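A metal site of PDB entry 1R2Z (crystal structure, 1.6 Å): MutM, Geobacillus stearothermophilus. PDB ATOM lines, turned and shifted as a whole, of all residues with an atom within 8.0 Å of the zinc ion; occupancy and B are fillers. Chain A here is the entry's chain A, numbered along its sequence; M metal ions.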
ATOM      1  N   PHE A 182     -27.647  30.028 -16.290  1.00  0.00           N
ATOM      2  CA  PHE A 182     -26.386  29.300 -16.162  1.00  0.00           C
ATOM      3  C   PHE A 182     -25.252  30.282 -15.917  1.00  0.00           C
ATOM      4  O   PHE A 182     -24.450  30.108 -15.004  1.00  0.00           O
ATOM      5  CB  PHE A 182     -26.056  28.519 -17.439  1.00  0.00           C
ATOM      6  CG  PHE A 182     -24.638  28.004 -17.469  1.00  0.00           C
ATOM      7  CD1 PHE A 182     -24.296  26.839 -16.794  1.00  0.00           C
ATOM      8  CD2 PHE A 182     -23.638  28.736 -18.100  1.00  0.00           C
ATOM      9  CE1 PHE A 182     -22.970  26.401 -16.761  1.00  0.00           C
ATOM     10  CE2 PHE A 182     -22.307  28.315 -18.081  1.00  0.00           C
ATOM     11  CZ  PHE A 182     -21.965  27.141 -17.403  1.00  0.00           C
ATOM     12  N   TYR A 240     -24.236  27.497 -23.551  1.00  0.00           N
ATOM     13  CA  TYR A 240     -23.631  26.730 -22.472  1.00  0.00           C
ATOM     14  C   TYR A 240     -24.489  25.549 -22.047  1.00  0.00           C
ATOM     15  O   TYR A 240     -23.967  24.500 -21.667  1.00  0.00           O
ATOM     16  CB  TYR A 240     -23.420  27.619 -21.246  1.00  0.00           C
ATOM     17  CG  TYR A 240     -22.288  28.592 -21.376  1.00  0.00           C
ATOM     18  CD1 TYR A 240     -20.959  28.173 -21.319  1.00  0.00           C
ATOM     19  CD2 TYR A 240     -22.536  29.958 -21.567  1.00  0.00           C
ATOM     20  CE1 TYR A 240     -19.910  29.069 -21.440  1.00  0.00           C
ATOM     21  CE2 TYR A 240     -21.496  30.860 -21.696  1.00  0.00           C
ATOM     22  CZ  TYR A 240     -20.186  30.410 -21.634  1.00  0.00           C
ATOM     23  OH  TYR A 240     -19.145  31.303 -21.760  1.00  0.00           O
ATOM     24  N   VAL A 241     -25.810  25.716 -22.132  1.00  0.00           N
ATOM     25  CA  VAL A 241     -26.697  24.642 -21.695  1.00  0.00           C
ATOM     26  C   VAL A 241     -27.885  24.284 -22.593  1.00  0.00           C
ATOM     27  O   VAL A 241     -28.256  23.113 -22.661  1.00  0.00           O
ATOM     28  CB  VAL A 241     -27.259  24.933 -20.282  1.00  0.00           C
ATOM     29  CG1 VAL A 241     -26.123  24.989 -19.264  1.00  0.00           C
ATOM     30  CG2 VAL A 241     -28.042  26.245 -20.290  1.00  0.00           C
ATOM     31  N   PRO A 248     -20.851  17.485 -21.768  1.00  0.00           N
ATOM     32  CA  PRO A 248     -20.138  18.108 -20.663  1.00  0.00           C
ATOM     33  C   PRO A 248     -20.278  19.627 -20.606  1.00  0.00           C
ATOM     34  O   PRO A 248     -20.286  20.307 -21.641  1.00  0.00           O
ATOM     35  CB  PRO A 248     -18.690  17.674 -20.899  1.00  0.00           C
ATOM     36  CG  PRO A 248     -18.615  17.558 -22.374  1.00  0.00           C
ATOM     37  CD  PRO A 248     -19.917  16.886 -22.731  1.00  0.00           C
ATOM     38  N   CYS A 249     -20.389  20.152 -19.388  1.00  0.00           N
ATOM     39  CA  CYS A 249     -20.476  21.586 -19.189  1.00  0.00           C
ATOM     40  C   CYS A 249     -19.180  22.179 -19.734  1.00  0.00           C
ATOM     41  O   CYS A 249     -18.102  21.623 -19.524  1.00  0.00           O
ATOM     42  CB  CYS A 249     -20.597  21.903 -17.701  1.00  0.00           C
ATOM     43  SG  CYS A 249     -20.530  23.658 -17.303  1.00  0.00           S
ATOM     44  N   LYS A 250     -19.281  23.312 -20.434  1.00  0.00           N
ATOM     45  CA  LYS A 250     -18.111  23.952 -20.998  1.00  0.00           C
ATOM     46  C   LYS A 250     -17.183  24.555 -19.942  1.00  0.00           C
ATOM     47  O   LYS A 250     -16.025  24.854 -20.228  1.00  0.00           O
ATOM     48  CB  LYS A 250     -18.530  25.050 -21.986  1.00  0.00           C
ATOM     49  CG  LYS A 250     -19.272  24.543 -23.210  1.00  0.00           C
ATOM     50  CD  LYS A 250     -19.555  25.674 -24.192  1.00  0.00           C
ATOM     51  CE  LYS A 250     -20.212  25.158 -25.463  1.00  0.00           C
ATOM     52  NZ  LYS A 250     -20.490  26.265 -26.422  1.00  0.00           N
ATOM     53  N   ARG A 251     -17.695  24.729 -18.730  1.00  0.00           N
ATOM     54  CA  ARG A 251     -16.914  25.317 -17.653  1.00  0.00           C
ATOM     55  C   ARG A 251     -16.378  24.334 -16.633  1.00  0.00           C
ATOM     56  O   ARG A 251     -15.258  24.496 -16.148  1.00  0.00           O
ATOM     57  CB  ARG A 251     -17.740  26.393 -16.932  1.00  0.00           C
ATOM     58  CG  ARG A 251     -18.041  27.604 -17.795  1.00  0.00           C
ATOM     59  N   CYS A 252     -17.166  23.311 -16.289  1.00  0.00           N
ATOM     60  CA  CYS A 252     -16.726  22.348 -15.283  1.00  0.00           C
ATOM     61  C   CYS A 252     -16.694  20.898 -15.740  1.00  0.00           C
ATOM     62  O   CYS A 252     -16.228  20.025 -15.011  1.00  0.00           O
ATOM     63  CB  CYS A 252     -17.588  22.458 -14.027  1.00  0.00           C
ATOM     64  SG  CYS A 252     -19.256  21.774 -14.210  1.00  0.00           S
ATOM     65  N   GLY A 253     -17.220  20.622 -16.925  1.00  0.00           N
ATOM     66  CA  GLY A 253     -17.206  19.260 -17.432  1.00  0.00           C
ATOM     67  C   GLY A 253     -18.310  18.334 -16.945  1.00  0.00           C
ATOM     68  O   GLY A 253     -18.425  17.205 -17.422  1.00  0.00           O
ATOM     69  N   THR A 254     -19.124  18.806 -16.010  1.00  0.00           N
ATOM     70  CA  THR A 254     -20.226  17.998 -15.488  1.00  0.00           C
ATOM     71  C   THR A 254     -21.300  17.902 -16.577  1.00  0.00           C
ATOM     72  O   THR A 254     -21.576  18.887 -17.268  1.00  0.00           O
ATOM     73  CB  THR A 254     -20.851  18.662 -14.240  1.00  0.00           C
ATOM     74  OG1 THR A 254     -19.840  18.803 -13.225  1.00  0.00           O
ATOM     75  CG2 THR A 254     -22.007  17.825 -13.700  1.00  0.00           C
ATOM     76  N   PRO A 255     -21.909  16.720 -16.749  1.00  0.00           N
ATOM     77  CA  PRO A 255     -22.951  16.584 -17.776  1.00  0.00           C
ATOM     78  C   PRO A 255     -24.127  17.519 -17.558  1.00  0.00           C
ATOM     79  O   PRO A 255     -24.661  17.626 -16.448  1.00  0.00           O
ATOM     80  CB  PRO A 255     -23.360  15.117 -17.677  1.00  0.00           C
ATOM     81  CG  PRO A 255     -22.105  14.438 -17.179  1.00  0.00           C
ATOM     82  CD  PRO A 255     -21.629  15.408 -16.120  1.00  0.00           C
ATOM     83  N   ILE A 256     -24.540  18.214 -18.611  1.00  0.00           N
ATOM     84  CA  ILE A 256     -25.672  19.117 -18.531  1.00  0.00           C
ATOM     85  C   ILE A 256     -26.923  18.252 -18.368  1.00  0.00           C
ATOM     86  O   ILE A 256     -27.022  17.178 -18.965  1.00  0.00           O
ATOM     87  CB  ILE A 256     -25.779  19.986 -19.797  1.00  0.00           C
ATOM     88  CG1 ILE A 256     -24.522  20.856 -19.918  1.00  0.00           C
ATOM     89  CG2 ILE A 256     -27.046  20.844 -19.758  1.00  0.00           C
ATOM     90  CD1 ILE A 256     -24.191  21.676 -18.672  1.00  0.00           C
ATOM     91  N   TYR A 268     -29.589  22.850 -17.502  1.00  0.00           N
ATOM     92  CA  TYR A 268     -28.748  23.482 -16.495  1.00  0.00           C
ATOM     93  C   TYR A 268     -27.564  22.591 -16.110  1.00  0.00           C
ATOM     94  O   TYR A 268     -27.565  21.402 -16.380  1.00  0.00           O
ATOM     95  CB  TYR A 268     -29.593  23.751 -15.243  1.00  0.00           C
ATOM     96  CG  TYR A 268     -30.099  22.479 -14.599  1.00  0.00           C
ATOM     97  CD1 TYR A 268     -29.372  21.845 -13.592  1.00  0.00           C
ATOM     98  CD2 TYR A 268     -31.267  21.870 -15.051  1.00  0.00           C
ATOM     99  CE1 TYR A 268     -29.796  20.629 -13.055  1.00  0.00           C
ATOM    100  CE2 TYR A 268     -31.707  20.649 -14.525  1.00  0.00           C
ATOM    101  CZ  TYR A 268     -30.954  20.034 -13.528  1.00  0.00           C
ATOM    102  OH  TYR A 268     -31.361  18.821 -13.018  1.00  0.00           O
ATOM    103  N   CYS A 269     -26.562  23.201 -15.491  1.00  0.00           N
ATOM    104  CA  CYS A 269     -25.420  22.449 -14.996  1.00  0.00           C
ATOM    105  C   CYS A 269     -25.643  22.363 -13.490  1.00  0.00           C
ATOM    106  O   CYS A 269     -25.723  23.387 -12.810  1.00  0.00           O
ATOM    107  CB  CYS A 269     -24.104  23.168 -15.263  1.00  0.00           C
ATOM    108  SG  CYS A 269     -22.758  22.311 -14.400  1.00  0.00           S
ATOM    109  N   PRO A 270     -25.738  21.140 -12.955  1.00  0.00           N
ATOM    110  CA  PRO A 270     -25.964  20.944 -11.524  1.00  0.00           C
ATOM    111  C   PRO A 270     -24.833  21.419 -10.612  1.00  0.00           C
ATOM    112  O   PRO A 270     -25.023  21.565  -9.402  1.00  0.00           O
ATOM    113  CB  PRO A 270     -26.234  19.449 -11.413  1.00  0.00           C
ATOM    114  CG  PRO A 270     -25.369  18.882 -12.489  1.00  0.00           C
ATOM    115  CD  PRO A 270     -25.582  19.844 -13.643  1.00  0.00           C
ATOM    116  N   ARG A 271     -23.654  21.658 -11.176  1.00  0.00           N
ATOM    117  CA  ARG A 271     -22.528  22.125 -10.381  1.00  0.00           C
ATOM    118  C   ARG A 271     -22.342  23.653 -10.438  1.00  0.00           C
ATOM    119  O   ARG A 271     -22.177  24.297  -9.400  1.00  0.00           O
ATOM    120  CB  ARG A 271     -21.237  21.441 -10.825  1.00  0.00           C
ATOM    121  CG  ARG A 271     -19.998  21.992 -10.122  1.00  0.00           C
ATOM    122  CD  ARG A 271     -18.737  21.204 -10.458  1.00  0.00           C
ATOM    123  NE  ARG A 271     -17.607  21.687  -9.677  1.00  0.00           N
ATOM    124  CZ  ARG A 271     -16.404  21.137  -9.670  1.00  0.00           C
ATOM    125  NH1 ARG A 271     -15.443  21.652  -8.913  1.00  0.00           N
ATOM    126  NH2 ARG A 271     -16.149  20.071 -10.422  1.00  0.00           N
ATOM    127  N   CYS A 272     -22.382  24.223 -11.634  1.00  0.00           N
ATOM    128  CA  CYS A 272     -22.205  25.661 -11.801  1.00  0.00           C
ATOM    129  C   CYS A 272     -23.383  26.499 -11.299  1.00  0.00           C
ATOM    130  O   CYS A 272     -23.209  27.658 -10.939  1.00  0.00           O
ATOM    131  CB  CYS A 272     -21.953  26.015 -13.269  1.00  0.00           C
ATOM    132  SG  CYS A 272     -20.350  25.480 -13.939  1.00  0.00           S
ATOM    133  N   GLN A 273     -24.563  25.907 -11.286  1.00  0.00           N
ATOM    134  CA  GLN A 273     -25.762  26.609 -10.840  1.00  0.00           C
ATOM    135  C   GLN A 273     -26.219  26.122  -9.470  1.00  0.00           C
ATOM    136  O   GLN A 273     -26.280  24.924  -9.213  1.00  0.00           O
ATOM    137  CB  GLN A 273     -26.870  26.451 -11.887  1.00  0.00           C
ATOM    138  CG  GLN A 273     -26.559  27.167 -13.201  1.00  0.00           C
ATOM    139  CD  GLN A 273     -27.470  26.771 -14.340  1.00  0.00           C
ATOM    140  OE1 GLN A 273     -27.131  25.929 -15.166  1.00  0.00           O
ATOM    141  NE2 GLN A 273     -28.651  27.384 -14.387  1.00  0.00           N
HETATM  142 ZN    ZN M   1     -20.731  23.410 -14.958  1.00  0.00          ZN
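The zinc ion is bound by SG of Cys 252 (2.3 Å), SG of Cys 272 (2.3 Å), SG of Cys 249 (2.4 Å) and SG of Cys 269 (2.4 Å). The zinc ion has four donor atoms within binding distance.
Four residues have an atom within 4 Å of the zinc ion: Cys 249, Cys 252, Cys 269 and Cys 272.
N of Arg 271 sits close to SG of Cys 269, at 3.4 Å. The side-chain sulfur (SG) of Cys 252 sits close to the side-chain hydroxyl (OG1) of Thr 254, at 3.2 Å. The backbone NH of Cys 269 lies within hydrogen-bond range of the side-chain amide oxygen of Gln 273 (2.8 Å). SG of Cys 249 sits close to N of Arg 251. O of Thr 254 is in hydrogen-bond range of N of Cys 249 (2.7 Å).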
